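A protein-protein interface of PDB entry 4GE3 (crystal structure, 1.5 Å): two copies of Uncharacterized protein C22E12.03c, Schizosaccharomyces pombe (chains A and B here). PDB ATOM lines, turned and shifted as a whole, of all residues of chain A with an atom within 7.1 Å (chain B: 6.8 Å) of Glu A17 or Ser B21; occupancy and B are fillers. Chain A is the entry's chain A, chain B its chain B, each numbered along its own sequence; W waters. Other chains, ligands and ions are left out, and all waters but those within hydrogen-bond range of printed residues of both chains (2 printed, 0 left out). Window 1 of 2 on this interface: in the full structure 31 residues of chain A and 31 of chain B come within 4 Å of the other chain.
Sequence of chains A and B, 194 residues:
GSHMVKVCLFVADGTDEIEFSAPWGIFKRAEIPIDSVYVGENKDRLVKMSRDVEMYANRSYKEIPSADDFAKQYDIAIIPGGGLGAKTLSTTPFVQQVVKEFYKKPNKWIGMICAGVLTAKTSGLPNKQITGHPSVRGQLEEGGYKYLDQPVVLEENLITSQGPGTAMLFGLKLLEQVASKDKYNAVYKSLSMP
The guanidinium group (NH2) of Arg B29 is in salt-bridge range of the side-chain carboxylate (OD1) of Asp A16 (2.8 Å).
The side-chain hydroxyl of Ser A21 is in hydrogen-bond range of the side-chain hydroxyl of Ser B21.
The backbone carbonyl oxygen of Arg A51 sits at hydrogen-bond distance from the indole nitrogen of Trp B24 (2.8 Å).
OD2 of Asp A52 lies within salt-bridge range of NZ of Lys B28 (2.7 Å).
N of Ile A18 sits at hydrogen-bond distance from OD2 of Asp A16, 3.0 Å away.
OD2 of Asp A16 sits at hydrogen-bond distance from N of Glu A19, 2.9 Å away.
N of Asp A16 lies within hydrogen-bond range of O of Gly A81, at 2.9 Å.
OE2 of Glu A17 sits at hydrogen-bond distance from N of Asp A52, at 3.2 Å.
O of Glu B17 sits at hydrogen-bond distance from OG of Ser B21 (2.9 Å).
The guanidinium group (NH1) of Arg B29 lies within hydrogen-bond range of the backbone carbonyl oxygen (O) of Gly B25 (3.0 Å).
O of Glu A17 touches OG of Ser B21, 3.7 Å away.
Trp B24 touches Glu A17 (NE1 to OE2, 3.8 Å).
Arg B29 touches Ile A18.
Met B168 touches Ile A18.
OG of Ser A21 touches O of Glu B17, at 3.7 Å.
O of Ser A21 touches CG1 of Ile B18 (3.3 Å).
Arg B29 touches Arg A51 (CG to CZ, 3.6 Å).
CE1 of Phe B20 touches CG2 of Val A53 (3.95 Å).
SD of Met B55 touches CG1 of Val A53, at 3.9 Å.
Glu A54 touches Met B55 (O to CA, 3.3 Å).
Of the printed residues of chain B, Glu A17 touches Ser B21 and Trp B24.
Printed residues of chain A within 4 Å of Ser B21: Glu A17 (3.7 Å), Ile A18 (3.3 Å) and Ser A21 (2.8 Å).
Of the printed residues of chain B, Glu A54 touches Met B55 (3.3 Å).
Of the printed residues of chain A, Phe B20 touches Val A53 (3.95 Å).
Of the printed residues of chain A, Met B55 touches Val A53 and Glu A54.
Of the printed residues of chain A, Ala B22 touches Ile A18.
Lys A48 touches none of the printed residues of chain B.
The nearest printed residue of chain B that does not touch Glu A17 is Gly B25 (5.6 Å).
Hydrophobic or aromatic side chains of chain A within 4 Å of the printed part of chain B: Ile A18 and Val A53.
Along chain A the printed residues that touch a printed residue of chain B span positions 16 to 54.
Of the 18 printed residues of chain B, 10 touch a printed residue of chain A.
Among the printed residues, 19 pairs touch across the chains.
Glu A17 touches Ser B21, and with the chains exchanged Ser A21 touches Glu B17.
Ile A18 touches Ser B21, and with the chains exchanged Ser A21 touches Ile B18.
Ile A18 touches Ala B22, and with the chains exchanged Ala A22 touches Ile B18.
Ser A21 touches its own counterpart, Ser B21.
9 positions are printed for both chains.
Of the 19 pairs that touch across the chains among the printed residues, 7 have their exchanged pair printed and touching as well.
Water W1 lies within hydrogen-bond range of the side-chain carboxylate (OD1) of Asp A16 (2.7 Å), the side-chain hydroxyl (OG) of Ser A50 (2.7 Å), the guanidinium group (NE) of Arg A51 (3.0 Å) and the guanidinium group (NH2) of Arg B29 (3.3 Å).
Water W2 lies within hydrogen-bond range of OD1 of Asp A16 (2.7 Å), NH1 of Arg B29 (3.0 Å) and OE1 of Glu A17 (3.1 Å).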
ATOM      1  N   GLY A  14     -15.356  13.903  16.433  1.00  0.00           N
ATOM      2  CA  GLY A  14     -14.984  15.215  15.926  1.00  0.00           C
ATOM      3  C   GLY A  14     -15.988  16.295  16.273  1.00  0.00           C
ATOM      4  O   GLY A  14     -15.836  17.430  15.838  1.00  0.00           O
ATOM      5  N   THR A  15     -17.007  15.984  17.076  1.00  0.00           N
ATOM      6  CA  THR A  15     -17.921  17.032  17.536  1.00  0.00           C
ATOM      7  C   THR A  15     -17.246  17.958  18.540  1.00  0.00           C
ATOM      8  O   THR A  15     -16.525  17.510  19.446  1.00  0.00           O
ATOM      9  CB  THR A  15     -19.165  16.422  18.173  1.00  0.00           C
ATOM     10  OG1 THR A  15     -19.986  15.876  17.146  1.00  0.00           O
ATOM     11  CG2 THR A  15     -19.984  17.460  18.911  1.00  0.00           C
ATOM     12  N   ASP A  16     -17.506  19.259  18.409  1.00  0.00           N
ATOM     13  CA  ASP A  16     -16.915  20.239  19.317  1.00  0.00           C
ATOM     14  C   ASP A  16     -17.431  20.141  20.761  1.00  0.00           C
ATOM     15  O   ASP A  16     -18.630  20.130  20.966  1.00  0.00           O
ATOM     16  CB  ASP A  16     -17.145  21.655  18.781  1.00  0.00           C
ATOM     17  CG  ASP A  16     -16.472  22.673  19.655  1.00  0.00           C
ATOM     18  OD1 ASP A  16     -15.247  22.715  19.590  1.00  0.00           O
ATOM     19  OD2 ASP A  16     -17.161  23.382  20.414  1.00  0.00           O
ATOM     20  N   GLU A  17     -16.489  20.105  21.728  1.00  0.00           N
ATOM     21  CA  GLU A  17     -16.849  19.950  23.151  1.00  0.00           C
ATOM     22  C   GLU A  17     -17.698  21.113  23.643  1.00  0.00           C
ATOM     23  O   GLU A  17     -18.668  20.920  24.387  1.00  0.00           O
ATOM     24  CB  GLU A  17     -15.620  19.793  24.052  1.00  0.00           C
ATOM     25  CG  GLU A  17     -14.844  18.504  23.837  1.00  0.00           C
ATOM     26  CD  GLU A  17     -13.774  18.560  22.731  1.00  0.00           C
ATOM     27  OE1 GLU A  17     -13.838  19.391  21.770  1.00  0.00           O
ATOM     28  OE2 GLU A  17     -12.866  17.736  22.785  1.00  0.00           O
ATOM     29  N   ILE A  18     -17.313  22.331  23.271  1.00  0.00           N
ATOM     30  CA  ILE A  18     -18.010  23.517  23.785  1.00  0.00           C
ATOM     31  C   ILE A  18     -19.454  23.589  23.252  1.00  0.00           C
ATOM     32  O   ILE A  18     -20.398  23.858  24.013  1.00  0.00           O
ATOM     33  CB  ILE A  18     -17.204  24.786  23.424  1.00  0.00           C
ATOM     34  CG1 ILE A  18     -15.915  24.836  24.244  1.00  0.00           C
ATOM     35  CG2 ILE A  18     -18.055  26.043  23.668  1.00  0.00           C
ATOM     36  CD1 ILE A  18     -14.842  25.826  23.674  1.00  0.00           C
ATOM     37  N   GLU A  19     -19.610  23.333  21.952  1.00  0.00           N
ATOM     38  CA  GLU A  19     -20.918  23.423  21.349  1.00  0.00           C
ATOM     39  C   GLU A  19     -21.838  22.270  21.762  1.00  0.00           C
ATOM     40  O   GLU A  19     -23.055  22.425  21.743  1.00  0.00           O
ATOM     41  CB  GLU A  19     -20.778  23.499  19.827  1.00  0.00           C
ATOM     42  CG  GLU A  19     -20.049  24.787  19.408  1.00  0.00           C
ATOM     43  CD  GLU A  19     -19.481  24.771  18.041  1.00  0.00           C
ATOM     44  OE1 GLU A  19     -19.802  23.865  17.248  1.00  0.00           O
ATOM     45  OE2 GLU A  19     -18.739  25.729  17.765  1.00  0.00           O
ATOM     46  N   PHE A  20     -21.284  21.123  22.150  1.00  0.00           N
ATOM     47  CA  PHE A  20     -22.089  20.047  22.720  1.00  0.00           C
ATOM     48  C   PHE A  20     -22.499  20.458  24.142  1.00  0.00           C
ATOM     49  O   PHE A  20     -23.665  20.362  24.514  1.00  0.00           O
ATOM     50  CB  PHE A  20     -21.241  18.771  22.803  1.00  0.00           C
ATOM     51  CG  PHE A  20     -21.951  17.612  23.477  1.00  0.00           C
ATOM     52  CD1 PHE A  20     -21.974  17.505  24.866  1.00  0.00           C
ATOM     53  CD2 PHE A  20     -22.626  16.651  22.704  1.00  0.00           C
ATOM     54  CE1 PHE A  20     -22.683  16.430  25.505  1.00  0.00           C
ATOM     55  CE2 PHE A  20     -23.302  15.576  23.338  1.00  0.00           C
ATOM     56  CZ  PHE A  20     -23.345  15.500  24.740  1.00  0.00           C
ATOM     57  N   SER A  21     -21.552  20.950  24.937  1.00  0.00           N
ATOM     58  CA  SER A  21     -21.816  21.080  26.387  1.00  0.00           C
ATOM     59  C   SER A  21     -22.817  22.168  26.716  1.00  0.00           C
ATOM     60  O   SER A  21     -23.544  22.074  27.712  1.00  0.00           O
ATOM     61  CB  SER A  21     -20.531  21.328  27.163  1.00  0.00           C
ATOM     62  OG  SER A  21     -19.642  20.236  27.045  1.00  0.00           O
ATOM     63  N   ALA A  22     -22.847  23.225  25.918  1.00  0.00           N
ATOM     64  CA  ALA A  22     -23.755  24.354  26.223  1.00  0.00           C
ATOM     65  C   ALA A  22     -25.249  23.984  26.136  1.00  0.00           C
ATOM     66  O   ALA A  22     -25.959  24.068  27.136  1.00  0.00           O
ATOM     67  CB  ALA A  22     -23.398  25.574  25.379  1.00  0.00           C
ATOM     68  N   PRO A  23     -25.745  23.508  24.970  1.00  0.00           N
ATOM     69  CA  PRO A  23     -27.139  23.068  24.949  1.00  0.00           C
ATOM     70  C   PRO A  23     -27.398  21.895  25.914  1.00  0.00           C
ATOM     71  O   PRO A  23     -28.481  21.844  26.535  1.00  0.00           O
ATOM     72  CB  PRO A  23     -27.377  22.630  23.494  1.00  0.00           C
ATOM     73  CG  PRO A  23     -25.990  22.409  22.920  1.00  0.00           C
ATOM     74  CD  PRO A  23     -25.097  23.435  23.634  1.00  0.00           C
ATOM     75  N   LYS A  48     -14.743  10.190  20.339  1.00  0.00           N
ATOM     76  CA  LYS A  48     -13.556  11.046  20.416  1.00  0.00           C
ATOM     77  C   LYS A  48     -13.936  12.414  19.848  1.00  0.00           C
ATOM     78  O   LYS A  48     -14.132  12.575  18.634  1.00  0.00           O
ATOM     79  CB  LYS A  48     -12.400  10.415  19.632  1.00  0.00           C
ATOM     80  CG  LYS A  48     -11.140  11.270  19.674  1.00  0.00           C
ATOM     81  CD  LYS A  48      -9.992  10.628  18.924  1.00  0.00           C
ATOM     82  CE  LYS A  48      -8.710  11.395  19.219  1.00  0.00           C
ATOM     83  NZ  LYS A  48      -7.644  10.910  18.340  1.00  0.00           N
ATOM     84  N   MET A  49     -14.057  13.397  20.741  1.00  0.00           N
ATOM     85  CA  MET A  49     -14.534  14.728  20.399  1.00  0.00           C
ATOM     86  C   MET A  49     -13.455  15.513  19.652  1.00  0.00           C
ATOM     87  O   MET A  49     -12.299  15.094  19.590  1.00  0.00           O
ATOM     88  CB  MET A  49     -14.971  15.457  21.672  1.00  0.00           C
ATOM     89  CG  MET A  49     -16.075  14.689  22.442  1.00  0.00           C
ATOM     90  SD  MET A  49     -17.689  14.575  21.644  1.00  0.00           S
ATOM     91  CE  MET A  49     -18.412  16.172  22.005  1.00  0.00           C
ATOM     92  N   SER A  50     -13.854  16.668  19.118  1.00  0.00           N
ATOM     93  CA  SER A  50     -12.953  17.493  18.271  1.00  0.00           C
ATOM     94  C   SER A  50     -11.571  17.769  18.870  1.00  0.00           C
ATOM     95  O   SER A  50     -10.538  17.640  18.199  1.00  0.00           O
ATOM     96  CB  SER A  50     -13.668  18.794  17.911  1.00  0.00           C
ATOM     97  OG  SER A  50     -12.925  19.511  16.953  1.00  0.00           O
ATOM     98  N   ARG A  51     -11.581  18.136  20.149  1.00  0.00           N
ATOM     99  CA  ARG A  51     -10.386  18.476  20.868  1.00  0.00           C
ATOM    100  C   ARG A  51     -10.024  17.412  21.900  1.00  0.00           C
ATOM    101  O   ARG A  51      -9.394  17.700  22.927  1.00  0.00           O
ATOM    102  CB  ARG A  51     -10.514  19.858  21.511  1.00  0.00           C
ATOM    103  CG  ARG A  51     -11.063  20.976  20.569  1.00  0.00           C
ATOM    104  CD  ARG A  51     -10.055  21.291  19.450  1.00  0.00           C
ATOM    105  NE  ARG A  51     -10.639  22.201  18.460  1.00  0.00           N
ATOM    106  CZ  ARG A  51      -9.900  22.930  17.607  1.00  0.00           C
ATOM    107  NH1 ARG A  51      -8.582  22.904  17.654  1.00  0.00           N
ATOM    108  NH2 ARG A  51     -10.517  23.717  16.738  1.00  0.00           N
ATOM    109  N   ASP A  52     -10.364  16.166  21.565  1.00  0.00           N
ATOM    110  CA  ASP A  52      -9.777  14.964  22.180  1.00  0.00           C
ATOM    111  C   ASP A  52     -10.419  14.487  23.479  1.00  0.00           C
ATOM    112  O   ASP A  52      -9.922  13.518  24.065  1.00  0.00           O
ATOM    113  CB  ASP A  52      -8.257  15.089  22.349  1.00  0.00           C
ATOM    114  CG  ASP A  52      -7.591  15.468  21.064  1.00  0.00           C
ATOM    115  OD1 ASP A  52      -7.912  14.799  20.065  1.00  0.00           O
ATOM    116  OD2 ASP A  52      -6.751  16.402  21.069  1.00  0.00           O
ATOM    117  N   VAL A  53     -11.487  15.147  23.935  1.00  0.00           N
ATOM    118  CA  VAL A  53     -12.266  14.548  25.031  1.00  0.00           C
ATOM    119  C   VAL A  53     -12.861  13.218  24.565  1.00  0.00           C
ATOM    120  O   VAL A  53     -13.331  13.100  23.416  1.00  0.00           O
ATOM    121  CB  VAL A  53     -13.364  15.495  25.535  1.00  0.00           C
ATOM    122  CG1 VAL A  53     -14.441  14.726  26.334  1.00  0.00           C
ATOM    123  CG2 VAL A  53     -12.726  16.619  26.365  1.00  0.00           C
ATOM    124  N   GLU A  54     -12.781  12.192  25.414  1.00  0.00           N
ATOM    125  CA  GLU A  54     -13.454  10.932  25.135  1.00  0.00           C
ATOM    126  C   GLU A  54     -14.648  10.803  26.060  1.00  0.00           C
ATOM    127  O   GLU A  54     -14.496  10.819  27.279  1.00  0.00           O
ATOM    128  CB  GLU A  54     -12.484   9.739  25.246  1.00  0.00           C
ATOM    129  CG  GLU A  54     -11.353   9.866  24.205  1.00  0.00           C
ATOM    130  CD  GLU A  54     -10.342   8.743  24.217  1.00  0.00           C
ATOM    131  OE1 GLU A  54     -10.708   7.599  24.504  1.00  0.00           O
ATOM    132  OE2 GLU A  54      -9.155   8.992  23.900  1.00  0.00           O
ATOM    133  N   GLY A  81     -21.160  21.690  15.945  1.00  0.00           N
ATOM    134  CA  GLY A  81     -20.053  21.813  14.976  1.00  0.00           C
ATOM    135  C   GLY A  81     -18.799  21.061  15.395  1.00  0.00           C
ATOM    136  O   GLY A  81     -18.872  20.002  16.019  1.00  0.00           O
ATOM    137  N   GLY A  82     -17.652  21.616  15.039  1.00  0.00           N
ATOM    138  CA  GLY A  82     -16.382  20.902  15.012  1.00  0.00           C
ATOM    139  C   GLY A  82     -16.263  20.394  13.569  1.00  0.00           C
ATOM    140  O   GLY A  82     -17.247  19.827  13.041  1.00  0.00           O
ATOM    141  N   LEU B   9      -6.336  20.844  34.067  1.00  0.00           N
ATOM    142  CA  LEU B   9      -7.734  21.098  34.325  1.00  0.00           C
ATOM    143  C   LEU B   9      -8.225  20.024  35.295  1.00  0.00           C
ATOM    144  O   LEU B   9      -8.364  18.856  34.921  1.00  0.00           O
ATOM    145  CB  LEU B   9      -8.494  21.084  32.996  1.00  0.00           C
ATOM    146  CG  LEU B   9      -9.989  21.391  32.957  1.00  0.00           C
ATOM    147  CD1 LEU B   9     -10.487  22.551  33.781  1.00  0.00           C
ATOM    148  CD2 LEU B   9     -10.501  21.535  31.526  1.00  0.00           C
ATOM    149  N   ASP B  16     -18.945  20.631  36.355  1.00  0.00           N
ATOM    150  CA  ASP B  16     -19.815  21.173  35.327  1.00  0.00           C
ATOM    151  C   ASP B  16     -19.220  21.019  33.912  1.00  0.00           C
ATOM    152  O   ASP B  16     -18.056  21.365  33.674  1.00  0.00           O
ATOM    153  CB  ASP B  16     -20.051  22.651  35.585  1.00  0.00           C
ATOM    154  CG  ASP B  16     -21.017  23.236  34.578  1.00  0.00           C
ATOM    155  OD1 ASP B  16     -22.209  22.879  34.663  1.00  0.00           O
ATOM    156  OD2 ASP B  16     -20.552  23.984  33.677  1.00  0.00           O
ATOM    157  N   GLU B  17     -20.023  20.475  32.998  1.00  0.00           N
ATOM    158  CA  GLU B  17     -19.583  20.230  31.624  1.00  0.00           C
ATOM    159  C   GLU B  17     -19.195  21.512  30.924  1.00  0.00           C
ATOM    160  O   GLU B  17     -18.228  21.556  30.154  1.00  0.00           O
ATOM    161  CB  GLU B  17     -20.711  19.590  30.836  1.00  0.00           C
ATOM    162  CG  GLU B  17     -21.038  18.135  31.212  1.00  0.00           C
ATOM    163  CD  GLU B  17     -22.055  17.976  32.341  1.00  0.00           C
ATOM    164  OE1 GLU B  17     -22.301  18.941  33.128  1.00  0.00           O
ATOM    165  OE2 GLU B  17     -22.647  16.892  32.416  1.00  0.00           O
ATOM    166  N   ILE B  18     -19.976  22.575  31.102  1.00  0.00           N
ATOM    167  CA  ILE B  18     -19.695  23.810  30.359  1.00  0.00           C
ATOM    168  C   ILE B  18     -18.373  24.447  30.821  1.00  0.00           C
ATOM    169  O   ILE B  18     -17.548  24.880  30.001  1.00  0.00           O
ATOM    170  CB  ILE B  18     -20.865  24.787  30.525  1.00  0.00           C
ATOM    171  CG1 ILE B  18     -22.108  24.243  29.788  1.00  0.00           C
ATOM    172  CG2 ILE B  18     -20.535  26.219  29.993  1.00  0.00           C
ATOM    173  CD1 ILE B  18     -23.432  24.890  30.195  1.00  0.00           C
ATOM    174  N   GLU B  19     -18.192  24.488  32.145  1.00  0.00           N
ATOM    175  CA  GLU B  19     -16.992  25.084  32.715  1.00  0.00           C
ATOM    176  C   GLU B  19     -15.739  24.283  32.462  1.00  0.00           C
ATOM    177  O   GLU B  19     -14.663  24.844  32.393  1.00  0.00           O
ATOM    178  CB  GLU B  19     -17.208  25.355  34.208  1.00  0.00           C
ATOM    179  CG  GLU B  19     -18.307  26.385  34.392  1.00  0.00           C
ATOM    180  CD  GLU B  19     -18.872  26.430  35.787  1.00  0.00           C
ATOM    181  OE1 GLU B  19     -18.325  25.826  36.726  1.00  0.00           O
ATOM    182  OE2 GLU B  19     -19.937  27.077  35.905  1.00  0.00           O
ATOM    183  N   PHE B  20     -15.886  22.960  32.306  1.00  0.00           N
ATOM    184  CA  PHE B  20     -14.754  22.143  31.862  1.00  0.00           C
ATOM    185  C   PHE B  20     -14.435  22.447  30.374  1.00  0.00           C
ATOM    186  O   PHE B  20     -13.297  22.723  30.019  1.00  0.00           O
ATOM    187  CB  PHE B  20     -15.060  20.662  32.081  1.00  0.00           C
ATOM    188  CG  PHE B  20     -13.976  19.753  31.606  1.00  0.00           C
ATOM    189  CD1 PHE B  20     -13.861  19.436  30.239  1.00  0.00           C
ATOM    190  CD2 PHE B  20     -13.058  19.208  32.513  1.00  0.00           C
ATOM    191  CE1 PHE B  20     -12.830  18.610  29.777  1.00  0.00           C
ATOM    192  CE2 PHE B  20     -12.046  18.341  32.070  1.00  0.00           C
ATOM    193  CZ  PHE B  20     -11.919  18.045  30.699  1.00  0.00           C
ATOM    194  N   SER B  21     -15.466  22.430  29.543  1.00  0.00           N
ATOM    195  CA  SER B  21     -15.262  22.460  28.094  1.00  0.00           C
ATOM    196  C   SER B  21     -14.671  23.756  27.558  1.00  0.00           C
ATOM    197  O   SER B  21     -13.899  23.729  26.587  1.00  0.00           O
ATOM    198  CB  SER B  21     -16.568  22.096  27.376  1.00  0.00           C
ATOM    199  OG  SER B  21     -16.961  20.760  27.692  1.00  0.00           O
ATOM    200  N   ALA B  22     -14.999  24.886  28.193  1.00  0.00           N
ATOM    201  CA  ALA B  22     -14.530  26.183  27.672  1.00  0.00           C
ATOM    202  C   ALA B  22     -13.011  26.307  27.748  1.00  0.00           C
ATOM    203  O   ALA B  22     -12.332  26.447  26.694  1.00  0.00           O
ATOM    204  CB  ALA B  22     -15.230  27.307  28.364  1.00  0.00           C
ATOM    205  N   PRO B  23     -12.400  26.213  28.955  1.00  0.00           N
ATOM    206  CA  PRO B  23     -10.933  26.256  28.987  1.00  0.00           C
ATOM    207  C   PRO B  23     -10.262  25.096  28.229  1.00  0.00           C
ATOM    208  O   PRO B  23      -9.226  25.275  27.605  1.00  0.00           O
ATOM    209  CB  PRO B  23     -10.590  26.192  30.487  1.00  0.00           C
ATOM    210  CG  PRO B  23     -11.848  25.637  31.143  1.00  0.00           C
ATOM    211  CD  PRO B  23     -12.996  26.121  30.300  1.00  0.00           C
ATOM    212  N   TRP B  24     -10.839  23.898  28.310  1.00  0.00           N
ATOM    213  CA  TRP B  24     -10.307  22.787  27.519  1.00  0.00           C
ATOM    214  C   TRP B  24     -10.186  23.175  26.036  1.00  0.00           C
ATOM    215  O   TRP B  24      -9.119  23.034  25.428  1.00  0.00           O
ATOM    216  CB  TRP B  24     -11.234  21.585  27.671  1.00  0.00           C
ATOM    217  CG  TRP B  24     -10.695  20.406  26.916  1.00  0.00           C
ATOM    218  CD1 TRP B  24     -11.034  20.002  25.652  1.00  0.00           C
ATOM    219  CD2 TRP B  24      -9.693  19.495  27.368  1.00  0.00           C
ATOM    220  NE1 TRP B  24     -10.324  18.876  25.302  1.00  0.00           N
ATOM    221  CE2 TRP B  24      -9.481  18.556  26.333  1.00  0.00           C
ATOM    222  CE3 TRP B  24      -8.974  19.355  28.567  1.00  0.00           C
ATOM    223  CZ2 TRP B  24      -8.591  17.488  26.468  1.00  0.00           C
ATOM    224  CZ3 TRP B  24      -8.089  18.305  28.686  1.00  0.00           C
ATOM    225  CH2 TRP B  24      -7.900  17.393  27.659  1.00  0.00           C
ATOM    226  N   GLY B  25     -11.313  23.613  25.443  1.00  0.00           N
ATOM    227  CA  GLY B  25     -11.331  23.926  23.993  1.00  0.00           C
ATOM    228  C   GLY B  25     -10.467  25.121  23.619  1.00  0.00           C
ATOM    229  O   GLY B  25      -9.901  25.184  22.516  1.00  0.00           O
ATOM    230  N   ILE B  26     -10.369  26.071  24.530  1.00  0.00           N
ATOM    231  CA  ILE B  26      -9.566  27.257  24.275  1.00  0.00           C
ATOM    232  C   ILE B  26      -8.074  26.914  24.261  1.00  0.00           C
ATOM    233  O   ILE B  26      -7.343  27.330  23.339  1.00  0.00           O
ATOM    234  CB  ILE B  26      -9.902  28.375  25.279  1.00  0.00           C
ATOM    235  CG1 ILE B  26     -11.308  28.895  24.961  1.00  0.00           C
ATOM    236  CG2 ILE B  26      -8.860  29.512  25.238  1.00  0.00           C
ATOM    237  CD1 ILE B  26     -11.908  29.740  26.094  1.00  0.00           C
ATOM    238  N   LYS B  28      -6.746  23.942  23.828  1.00  0.00           N
ATOM    239  CA  LYS B  28      -6.495  23.082  22.673  1.00  0.00           C
ATOM    240  C   LYS B  28      -6.331  23.896  21.405  1.00  0.00           C
ATOM    241  O   LYS B  28      -5.420  23.640  20.651  1.00  0.00           O
ATOM    242  CB  LYS B  28      -7.583  22.015  22.504  1.00  0.00           C
ATOM    243  CG  LYS B  28      -7.452  20.871  23.504  1.00  0.00           C
ATOM    244  CD  LYS B  28      -6.575  19.767  22.905  1.00  0.00           C
ATOM    245  CE  LYS B  28      -6.352  18.691  23.927  1.00  0.00           C
ATOM    246  NZ  LYS B  28      -5.682  17.531  23.290  1.00  0.00           N
ATOM    247  N   ARG B  29      -7.201  24.884  21.181  1.00  0.00           N
ATOM    248  CA  ARG B  29      -7.062  25.737  19.992  1.00  0.00           C
ATOM    249  C   ARG B  29      -5.742  26.506  19.974  1.00  0.00           C
ATOM    250  O   ARG B  29      -5.150  26.729  18.901  1.00  0.00           O
ATOM    251  CB  ARG B  29      -8.232  26.710  19.903  1.00  0.00           C
ATOM    252  CG  ARG B  29      -9.529  26.094  19.370  1.00  0.00           C
ATOM    253  CD  ARG B  29     -10.729  26.957  19.734  1.00  0.00           C
ATOM    254  NE  ARG B  29     -11.971  26.442  19.145  1.00  0.00           N
ATOM    255  CZ  ARG B  29     -12.695  25.441  19.658  1.00  0.00           C
ATOM    256  NH1 ARG B  29     -12.313  24.793  20.770  1.00  0.00           N
ATOM    257  NH2 ARG B  29     -13.804  25.044  19.041  1.00  0.00           N
ATOM    258  N   MET B  49     -20.075  13.716  35.079  1.00  0.00           N
ATOM    259  CA  MET B  49     -20.096  15.170  35.219  1.00  0.00           C
ATOM    260  C   MET B  49     -21.414  15.613  35.868  1.00  0.00           C
ATOM    261  O   MET B  49     -22.356  14.835  36.029  1.00  0.00           O
ATOM    262  CB  MET B  49     -19.868  15.809  33.855  1.00  0.00           C
ATOM    263  CG  MET B  49     -18.577  15.315  33.228  1.00  0.00           C
ATOM    264  SD  MET B  49     -17.067  15.880  33.992  1.00  0.00           S
ATOM    265  CE  MET B  49     -16.972  17.532  33.328  1.00  0.00           C
ATOM    266  N   MET B  55     -17.390  10.956  30.921  1.00  0.00           N
ATOM    267  CA  MET B  55     -16.179  11.166  30.132  1.00  0.00           C
ATOM    268  C   MET B  55     -14.932  10.714  30.883  1.00  0.00           C
ATOM    269  O   MET B  55     -14.915  10.689  32.122  1.00  0.00           O
ATOM    270  CB  MET B  55     -16.077  12.601  29.634  1.00  0.00           C
ATOM    271  CG  MET B  55     -15.852  13.581  30.702  1.00  0.00           C
ATOM    272  SD  MET B  55     -15.162  15.206  30.124  1.00  0.00           S
ATOM    273  CE  MET B  55     -14.174  15.448  31.550  1.00  0.00           C
ATOM    274  N   ALA B 167     -17.823  31.071  31.250  1.00  0.00           N
ATOM    275  CA  ALA B 167     -16.717  30.110  31.136  1.00  0.00           C
ATOM    276  C   ALA B 167     -15.792  30.399  29.964  1.00  0.00           C
ATOM    277  O   ALA B 167     -14.576  30.222  30.088  1.00  0.00           O
ATOM    278  CB  ALA B 167     -17.243  28.716  31.068  1.00  0.00           C
ATOM    279  N   MET B 168     -16.346  30.900  28.855  1.00  0.00           N
ATOM    280  CA  MET B 168     -15.498  31.324  27.731  1.00  0.00           C
ATOM    281  C   MET B 168     -14.613  32.515  28.078  1.00  0.00           C
ATOM    282  O   MET B 168     -13.402  32.515  27.780  1.00  0.00           O
ATOM    283  CB  MET B 168     -16.357  31.606  26.485  1.00  0.00           C
ATOM    284  CG  MET B 168     -17.027  30.337  25.877  1.00  0.00           C
ATOM    285  SD  MET B 168     -15.839  29.116  25.235  1.00  0.00           S
ATOM    286  CE  MET B 168     -15.281  29.922  23.716  1.00  0.00           C
HETATM  287  O   HOH W   1     -13.486  22.083  17.675  1.00  0.00           O
HETATM  288  O   HOH W   2     -13.887  22.516  21.951  1.00  0.00           O
